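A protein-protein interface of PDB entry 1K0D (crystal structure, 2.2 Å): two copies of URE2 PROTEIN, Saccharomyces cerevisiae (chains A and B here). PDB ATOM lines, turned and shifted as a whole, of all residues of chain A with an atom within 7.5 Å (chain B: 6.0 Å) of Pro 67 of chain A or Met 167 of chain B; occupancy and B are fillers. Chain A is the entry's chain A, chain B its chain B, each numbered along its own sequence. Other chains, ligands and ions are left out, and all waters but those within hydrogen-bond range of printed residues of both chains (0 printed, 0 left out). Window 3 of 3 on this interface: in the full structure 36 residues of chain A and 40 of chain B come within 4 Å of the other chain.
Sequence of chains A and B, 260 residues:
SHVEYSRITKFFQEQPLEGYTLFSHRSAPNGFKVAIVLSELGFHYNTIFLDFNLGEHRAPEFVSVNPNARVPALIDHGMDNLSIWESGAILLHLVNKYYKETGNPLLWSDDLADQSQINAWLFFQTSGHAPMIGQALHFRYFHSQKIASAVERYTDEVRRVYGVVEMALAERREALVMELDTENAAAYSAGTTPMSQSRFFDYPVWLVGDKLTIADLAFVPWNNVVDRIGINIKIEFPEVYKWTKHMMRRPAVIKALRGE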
ATOM      1  N   HIS A  57     -23.956  23.715  -1.115  1.00  0.00           N
ATOM      2  CA  HIS A  57     -23.649  22.447  -1.765  1.00  0.00           C
ATOM      3  C   HIS A  57     -24.126  22.404  -3.215  1.00  0.00           C
ATOM      4  O   HIS A  57     -23.909  21.420  -3.922  1.00  0.00           O
ATOM      5  CB  HIS A  57     -24.252  21.288  -0.960  1.00  0.00           C
ATOM      6  CG  HIS A  57     -25.730  21.395  -0.750  1.00  0.00           C
ATOM      7  ND1 HIS A  57     -26.392  22.604  -0.698  1.00  0.00           N
ATOM      8  CD2 HIS A  57     -26.670  20.444  -0.536  1.00  0.00           C
ATOM      9  CE1 HIS A  57     -27.674  22.392  -0.463  1.00  0.00           C
ATOM     10  NE2 HIS A  57     -27.870  21.090  -0.360  1.00  0.00           N
ATOM     11  N   PHE A  62     -18.386  23.714  -5.634  1.00  0.00           N
ATOM     12  CA  PHE A  62     -18.487  22.531  -4.787  1.00  0.00           C
ATOM     13  C   PHE A  62     -18.969  21.324  -5.572  1.00  0.00           C
ATOM     14  O   PHE A  62     -18.522  20.205  -5.334  1.00  0.00           O
ATOM     15  CB  PHE A  62     -19.429  22.751  -3.606  1.00  0.00           C
ATOM     16  CG  PHE A  62     -19.592  21.526  -2.748  1.00  0.00           C
ATOM     17  CD1 PHE A  62     -18.490  20.950  -2.122  1.00  0.00           C
ATOM     18  CD2 PHE A  62     -20.835  20.913  -2.609  1.00  0.00           C
ATOM     19  CE1 PHE A  62     -18.621  19.784  -1.373  1.00  0.00           C
ATOM     20  CE2 PHE A  62     -20.976  19.745  -1.861  1.00  0.00           C
ATOM     21  CZ  PHE A  62     -19.865  19.181  -1.243  1.00  0.00           C
ATOM     22  N   VAL A  63     -19.893  21.548  -6.499  1.00  0.00           N
ATOM     23  CA  VAL A  63     -20.396  20.456  -7.312  1.00  0.00           C
ATOM     24  C   VAL A  63     -19.239  19.911  -8.145  1.00  0.00           C
ATOM     25  O   VAL A  63     -19.301  18.788  -8.640  1.00  0.00           O
ATOM     26  CB  VAL A  63     -21.542  20.923  -8.230  1.00  0.00           C
ATOM     27  CG1 VAL A  63     -21.995  19.783  -9.131  1.00  0.00           C
ATOM     28  CG2 VAL A  63     -22.707  21.409  -7.380  1.00  0.00           C
ATOM     29  N   SER A  64     -18.181  20.708  -8.290  1.00  0.00           N
ATOM     30  CA  SER A  64     -16.999  20.281  -9.044  1.00  0.00           C
ATOM     31  C   SER A  64     -16.156  19.344  -8.189  1.00  0.00           C
ATOM     32  O   SER A  64     -15.358  18.564  -8.704  1.00  0.00           O
ATOM     33  CB  SER A  64     -16.147  21.485  -9.466  1.00  0.00           C
ATOM     34  OG  SER A  64     -16.693  22.121 -10.613  1.00  0.00           O
ATOM     35  N   VAL A  65     -16.337  19.434  -6.875  1.00  0.00           N
ATOM     36  CA  VAL A  65     -15.610  18.585  -5.938  1.00  0.00           C
ATOM     37  C   VAL A  65     -16.377  17.274  -5.807  1.00  0.00           C
ATOM     38  O   VAL A  65     -15.790  16.194  -5.840  1.00  0.00           O
ATOM     39  CB  VAL A  65     -15.504  19.256  -4.551  1.00  0.00           C
ATOM     40  CG1 VAL A  65     -14.794  18.332  -3.569  1.00  0.00           C
ATOM     41  CG2 VAL A  65     -14.752  20.567  -4.679  1.00  0.00           C
ATOM     42  N   ASN A  66     -17.694  17.385  -5.653  1.00  0.00           N
ATOM     43  CA  ASN A  66     -18.557  16.223  -5.540  1.00  0.00           C
ATOM     44  C   ASN A  66     -19.741  16.385  -6.488  1.00  0.00           C
ATOM     45  O   ASN A  66     -20.657  17.155  -6.219  1.00  0.00           O
ATOM     46  CB  ASN A  66     -19.074  16.053  -4.107  1.00  0.00           C
ATOM     47  CG  ASN A  66     -19.883  14.778  -3.935  1.00  0.00           C
ATOM     48  OD1 ASN A  66     -20.299  14.424  -2.827  1.00  0.00           O
ATOM     49  ND2 ASN A  66     -20.107  14.074  -5.042  1.00  0.00           N
ATOM     50  N   PRO A  67     -19.728  15.662  -7.620  1.00  0.00           N
ATOM     51  CA  PRO A  67     -20.833  15.765  -8.577  1.00  0.00           C
ATOM     52  C   PRO A  67     -22.175  15.372  -7.972  1.00  0.00           C
ATOM     53  O   PRO A  67     -23.229  15.691  -8.528  1.00  0.00           O
ATOM     54  CB  PRO A  67     -20.407  14.832  -9.706  1.00  0.00           C
ATOM     55  CG  PRO A  67     -19.565  13.806  -9.007  1.00  0.00           C
ATOM     56  CD  PRO A  67     -18.745  14.652  -8.051  1.00  0.00           C
ATOM     57  N   ASN A  68     -22.136  14.684  -6.834  1.00  0.00           N
ATOM     58  CA  ASN A  68     -23.361  14.256  -6.162  1.00  0.00           C
ATOM     59  C   ASN A  68     -23.908  15.380  -5.277  1.00  0.00           C
ATOM     60  O   ASN A  68     -25.005  15.271  -4.727  1.00  0.00           O
ATOM     61  CB  ASN A  68     -23.096  13.011  -5.309  1.00  0.00           C
ATOM     62  CG  ASN A  68     -24.371  12.361  -4.817  1.00  0.00           C
ATOM     63  OD1 ASN A  68     -24.397  11.761  -3.744  1.00  0.00           O
ATOM     64  ND2 ASN A  68     -25.433  12.461  -5.606  1.00  0.00           N
ATOM     65  N   ALA A  69     -23.134  16.455  -5.138  1.00  0.00           N
ATOM     66  CA  ALA A  69     -23.542  17.608  -4.333  1.00  0.00           C
ATOM     67  C   ALA A  69     -23.941  17.229  -2.912  1.00  0.00           C
ATOM     68  O   ALA A  69     -24.939  17.721  -2.386  1.00  0.00           O
ATOM     69  CB  ALA A  69     -24.696  18.337  -5.013  1.00  0.00           C
ATOM     70  N   ARG A  70     -23.151  16.356  -2.293  1.00  0.00           N
ATOM     71  CA  ARG A  70     -23.413  15.915  -0.930  1.00  0.00           C
ATOM     72  C   ARG A  70     -22.125  15.939  -0.100  1.00  0.00           C
ATOM     73  O   ARG A  70     -21.022  16.074  -0.637  1.00  0.00           O
ATOM     74  CB  ARG A  70     -23.978  14.494  -0.949  1.00  0.00           C
ATOM     75  CG  ARG A  70     -25.341  14.363  -1.620  1.00  0.00           C
ATOM     76  CD  ARG A  70     -26.452  14.816  -0.690  1.00  0.00           C
ATOM     77  NE  ARG A  70     -27.770  14.749  -1.319  1.00  0.00           N
ATOM     78  CZ  ARG A  70     -28.201  15.594  -2.251  1.00  0.00           C
ATOM     79  NH1 ARG A  70     -27.421  16.583  -2.673  1.00  0.00           N
ATOM     80  NH2 ARG A  70     -29.415  15.452  -2.759  1.00  0.00           N
ATOM     81  N   SER A  83      -9.788  15.595  -5.664  1.00  0.00           N
ATOM     82  CA  SER A  83     -11.057  15.600  -4.953  1.00  0.00           C
ATOM     83  C   SER A  83     -11.622  14.186  -4.783  1.00  0.00           C
ATOM     84  O   SER A  83     -11.687  13.412  -5.737  1.00  0.00           O
ATOM     85  CB  SER A  83     -12.070  16.468  -5.695  1.00  0.00           C
ATOM     86  OG  SER A  83     -13.334  16.369  -5.076  1.00  0.00           O
ATOM     87  N   TRP A  85     -14.968  12.077  -3.098  1.00  0.00           N
ATOM     88  CA  TRP A  85     -16.298  12.134  -2.489  1.00  0.00           C
ATOM     89  C   TRP A  85     -16.786  10.721  -2.137  1.00  0.00           C
ATOM     90  O   TRP A  85     -16.260   9.736  -2.656  1.00  0.00           O
ATOM     91  CB  TRP A  85     -17.282  12.833  -3.433  1.00  0.00           C
ATOM     92  CG  TRP A  85     -17.206  12.360  -4.842  1.00  0.00           C
ATOM     93  CD1 TRP A  85     -16.176  12.556  -5.721  1.00  0.00           C
ATOM     94  CD2 TRP A  85     -18.195  11.604  -5.546  1.00  0.00           C
ATOM     95  NE1 TRP A  85     -16.466  11.969  -6.927  1.00  0.00           N
ATOM     96  CE2 TRP A  85     -17.698  11.378  -6.849  1.00  0.00           C
ATOM     97  CE3 TRP A  85     -19.456  11.098  -5.205  1.00  0.00           C
ATOM     98  CZ2 TRP A  85     -18.419  10.665  -7.814  1.00  0.00           C
ATOM     99  CZ3 TRP A  85     -20.175  10.387  -6.165  1.00  0.00           C
ATOM    100  CH2 TRP A  85     -19.652  10.180  -7.454  1.00  0.00           C
ATOM    101  N   TRP B 121     -17.242   6.417  -7.376  1.00  0.00           N
ATOM    102  CA  TRP B 121     -18.378   5.998  -8.191  1.00  0.00           C
ATOM    103  C   TRP B 121     -18.936   4.665  -7.710  1.00  0.00           C
ATOM    104  O   TRP B 121     -20.151   4.461  -7.708  1.00  0.00           O
ATOM    105  CB  TRP B 121     -17.976   5.876  -9.659  1.00  0.00           C
ATOM    106  CG  TRP B 121     -17.752   7.197 -10.302  1.00  0.00           C
ATOM    107  CD1 TRP B 121     -16.553   7.750 -10.645  1.00  0.00           C
ATOM    108  CD2 TRP B 121     -18.755   8.166 -10.638  1.00  0.00           C
ATOM    109  NE1 TRP B 121     -16.747   9.004 -11.171  1.00  0.00           N
ATOM    110  CE2 TRP B 121     -18.087   9.286 -11.178  1.00  0.00           C
ATOM    111  CE3 TRP B 121     -20.152   8.196 -10.531  1.00  0.00           C
ATOM    112  CZ2 TRP B 121     -18.770  10.432 -11.614  1.00  0.00           C
ATOM    113  CZ3 TRP B 121     -20.832   9.333 -10.964  1.00  0.00           C
ATOM    114  CH2 TRP B 121     -20.137  10.436 -11.499  1.00  0.00           C
ATOM    115  N   ARG B 160     -32.536  11.704 -10.003  1.00  0.00           N
ATOM    116  CA  ARG B 160     -31.515  12.644  -9.586  1.00  0.00           C
ATOM    117  C   ARG B 160     -30.126  12.004  -9.711  1.00  0.00           C
ATOM    118  O   ARG B 160     -29.220  12.594 -10.297  1.00  0.00           O
ATOM    119  CB  ARG B 160     -31.764  13.081  -8.139  1.00  0.00           C
ATOM    120  CG  ARG B 160     -30.685  13.998  -7.586  1.00  0.00           C
ATOM    121  CD  ARG B 160     -30.749  14.084  -6.078  1.00  0.00           C
ATOM    122  NE  ARG B 160     -29.462  14.501  -5.546  1.00  0.00           N
ATOM    123  CZ  ARG B 160     -28.520  13.675  -5.100  1.00  0.00           C
ATOM    124  NH1 ARG B 160     -28.709  12.366  -5.098  1.00  0.00           N
ATOM    125  NH2 ARG B 160     -27.365  14.169  -4.680  1.00  0.00           N
ATOM    126  N   TYR B 162     -29.272   9.531 -11.534  1.00  0.00           N
ATOM    127  CA  TYR B 162     -28.976   9.268 -12.935  1.00  0.00           C
ATOM    128  C   TYR B 162     -28.548  10.560 -13.614  1.00  0.00           C
ATOM    129  O   TYR B 162     -27.768  10.544 -14.559  1.00  0.00           O
ATOM    130  CB  TYR B 162     -30.176   8.641 -13.656  1.00  0.00           C
ATOM    131  CG  TYR B 162     -30.099   7.126 -13.667  1.00  0.00           C
ATOM    132  CD1 TYR B 162     -30.771   6.365 -12.715  1.00  0.00           C
ATOM    133  CD2 TYR B 162     -29.291   6.463 -14.583  1.00  0.00           C
ATOM    134  CE1 TYR B 162     -30.639   4.981 -12.672  1.00  0.00           C
ATOM    135  CE2 TYR B 162     -29.149   5.077 -14.551  1.00  0.00           C
ATOM    136  CZ  TYR B 162     -29.826   4.343 -13.591  1.00  0.00           C
ATOM    137  OH  TYR B 162     -29.687   2.971 -13.552  1.00  0.00           O
ATOM    138  N   GLY B 163     -29.045  11.685 -13.110  1.00  0.00           N
ATOM    139  CA  GLY B 163     -28.662  12.967 -13.669  1.00  0.00           C
ATOM    140  C   GLY B 163     -27.197  13.242 -13.361  1.00  0.00           C
ATOM    141  O   GLY B 163     -26.494  13.861 -14.159  1.00  0.00           O
ATOM    142  N   VAL B 164     -26.733  12.785 -12.196  1.00  0.00           N
ATOM    143  CA  VAL B 164     -25.335  12.971 -11.805  1.00  0.00           C
ATOM    144  C   VAL B 164     -24.446  12.185 -12.772  1.00  0.00           C
ATOM    145  O   VAL B 164     -23.399  12.670 -13.209  1.00  0.00           O
ATOM    146  CB  VAL B 164     -25.076  12.469 -10.361  1.00  0.00           C
ATOM    147  CG1 VAL B 164     -23.601  12.589 -10.017  1.00  0.00           C
ATOM    148  CG2 VAL B 164     -25.909  13.278  -9.378  1.00  0.00           C
ATOM    149  N   VAL B 165     -24.866  10.973 -13.111  1.00  0.00           N
ATOM    150  CA  VAL B 165     -24.103  10.144 -14.041  1.00  0.00           C
ATOM    151  C   VAL B 165     -24.135  10.753 -15.451  1.00  0.00           C
ATOM    152  O   VAL B 165     -23.116  10.805 -16.147  1.00  0.00           O
ATOM    153  CB  VAL B 165     -24.671   8.706 -14.102  1.00  0.00           C
ATOM    154  CG1 VAL B 165     -23.919   7.894 -15.137  1.00  0.00           C
ATOM    155  CG2 VAL B 165     -24.561   8.045 -12.727  1.00  0.00           C
ATOM    156  N   GLU B 166     -25.313  11.210 -15.863  1.00  0.00           N
ATOM    157  CA  GLU B 166     -25.488  11.821 -17.178  1.00  0.00           C
ATOM    158  C   GLU B 166     -24.549  13.020 -17.318  1.00  0.00           C
ATOM    159  O   GLU B 166     -23.808  13.129 -18.294  1.00  0.00           O
ATOM    160  CB  GLU B 166     -26.939  12.281 -17.352  1.00  0.00           C
ATOM    161  CG  GLU B 166     -27.232  12.920 -18.700  1.00  0.00           C
ATOM    162  CD  GLU B 166     -27.268  11.911 -19.836  1.00  0.00           C
ATOM    163  OE1 GLU B 166     -27.393  12.334 -21.007  1.00  0.00           O
ATOM    164  OE2 GLU B 166     -27.178  10.692 -19.563  1.00  0.00           O
ATOM    165  N   MET B 167     -24.590  13.913 -16.335  1.00  0.00           N
ATOM    166  CA  MET B 167     -23.752  15.108 -16.332  1.00  0.00           C
ATOM    167  C   MET B 167     -22.267  14.747 -16.447  1.00  0.00           C
ATOM    168  O   MET B 167     -21.552  15.293 -17.288  1.00  0.00           O
ATOM    169  CB  MET B 167     -24.017  15.918 -15.052  1.00  0.00           C
ATOM    170  CG  MET B 167     -23.111  17.131 -14.843  1.00  0.00           C
ATOM    171  SD  MET B 167     -23.664  18.221 -13.481  1.00  0.00           S
ATOM    172  CE  MET B 167     -23.197  17.245 -12.007  1.00  0.00           C
ATOM    173  N   ALA B 168     -21.804  13.828 -15.605  1.00  0.00           N
ATOM    174  CA  ALA B 168     -20.409  13.414 -15.638  1.00  0.00           C
ATOM    175  C   ALA B 168     -20.025  12.881 -17.020  1.00  0.00           C
ATOM    176  O   ALA B 168     -18.958  13.208 -17.544  1.00  0.00           O
ATOM    177  CB  ALA B 168     -20.148  12.356 -14.573  1.00  0.00           C
ATOM    178  N   LEU B 169     -20.890  12.059 -17.607  1.00  0.00           N
ATOM    179  CA  LEU B 169     -20.605  11.507 -18.932  1.00  0.00           C
ATOM    180  C   LEU B 169     -20.578  12.621 -19.982  1.00  0.00           C
ATOM    181  O   LEU B 169     -19.731  12.624 -20.877  1.00  0.00           O
ATOM    182  CB  LEU B 169     -21.649  10.449 -19.309  1.00  0.00           C
ATOM    183  CG  LEU B 169     -21.622   9.155 -18.489  1.00  0.00           C
ATOM    184  CD1 LEU B 169     -22.829   8.296 -18.840  1.00  0.00           C
ATOM    185  CD2 LEU B 169     -20.318   8.399 -18.760  1.00  0.00           C
ATOM    186  N   ALA B 170     -21.508  13.564 -19.865  1.00  0.00           N
ATOM    187  CA  ALA B 170     -21.577  14.692 -20.786  1.00  0.00           C
ATOM    188  C   ALA B 170     -20.288  15.505 -20.712  1.00  0.00           C
ATOM    189  O   ALA B 170     -19.731  15.889 -21.738  1.00  0.00           O
ATOM    190  CB  ALA B 170     -22.771  15.576 -20.444  1.00  0.00           C
ATOM    191  N   GLU B 171     -19.810  15.764 -19.498  1.00  0.00           N
ATOM    192  CA  GLU B 171     -18.578  16.533 -19.324  1.00  0.00           C
ATOM    193  C   GLU B 171     -17.368  15.815 -19.908  1.00  0.00           C
ATOM    194  O   GLU B 171     -16.472  16.458 -20.450  1.00  0.00           O
ATOM    195  CB  GLU B 171     -18.325  16.827 -17.846  1.00  0.00           C
ATOM    196  CG  GLU B 171     -19.362  17.732 -17.210  1.00  0.00           C
ATOM    197  CD  GLU B 171     -19.063  18.009 -15.750  1.00  0.00           C
ATOM    198  OE1 GLU B 171     -18.014  18.627 -15.468  1.00  0.00           O
ATOM    199  OE2 GLU B 171     -19.872  17.604 -14.887  1.00  0.00           O
ATOM    200  N   ARG B 172     -17.335  14.489 -19.791  1.00  0.00           N
ATOM    201  CA  ARG B 172     -16.220  13.711 -20.333  1.00  0.00           C
ATOM    202  C   ARG B 172     -16.204  13.852 -21.855  1.00  0.00           C
ATOM    203  O   ARG B 172     -15.144  13.919 -22.475  1.00  0.00           O
ATOM    204  CB  ARG B 172     -16.369  12.231 -19.986  1.00  0.00           C
ATOM    205  CG  ARG B 172     -16.428  11.910 -18.511  1.00  0.00           C
ATOM    206  CD  ARG B 172     -15.084  12.059 -17.843  1.00  0.00           C
ATOM    207  NE  ARG B 172     -15.176  11.648 -16.447  1.00  0.00           N
ATOM    208  CZ  ARG B 172     -15.897  12.282 -15.526  1.00  0.00           C
ATOM    209  NH1 ARG B 172     -16.589  13.369 -15.856  1.00  0.00           N
ATOM    210  NH2 ARG B 172     -15.938  11.822 -14.282  1.00  0.00           N
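N of Asn 68 of chain A sits close to ND2 of Asn 66 of chain A, at 2.8 Å.
OD1 of Asn 66 of chain A lies close to O of Arg 70 of chain A.
The guanidinium group (NH1) of Arg 70 of chain A sits close to the backbone carbonyl oxygen (O) of Asn 68 of chain A (3.4 Å).
Hydrophobic or aromatic side chains of chain B that line the printed part of chain A: Trp 121, Val 164 and Met 167.
Of the 12 printed residues of chain A, 4 touch a printed residue of chain B.
Hydrophobic or aromatic side chains of chain A that line the printed part of chain B: Pro 67 and Trp 85.
No position is printed for both chains.
Among the printed residues, merely in contact across the chains: Pro 67 of chain A with Val 164 of chain B (3.5 Å), Pro 67 of chain A with Met 167 of chain B (3.8 Å), Asn 68 of chain A with Val 164 of chain B (3.9 Å) and Trp 85 of chain A with Trp 121 of chain B (3.7 Å).
The backbone carbonyl oxygen (O) of Asn 68 of chain A lies within hydrogen-bond range of the guanidinium group (NH2) of Arg 160 of chain B.
The guanidinium group of Arg 70 of chain A lies close to the guanidinium group of Arg 160 of chain B (2.9 Å).
Pro 67 of chain A touches just these residues of chain B: Val 164 (3.5 Å) and Met 167 (3.8 Å).
Of the printed residues of chain A, Met 167 of chain B touches Pro 67 (3.8 Å).
Of the printed residues of chain B, Arg 70 of chain A touches Arg 160 (2.9 Å).
Printed residues of chain B within 4 Å of Asn 68 of chain A: Arg 160 and Val 164.
Of the printed residues of chain B, Trp 85 of chain A touches Trp 121.
The nearest printed residue of chain B that does not touch Arg 70 of chain A is Val 164 of chain B (7.6 Å).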
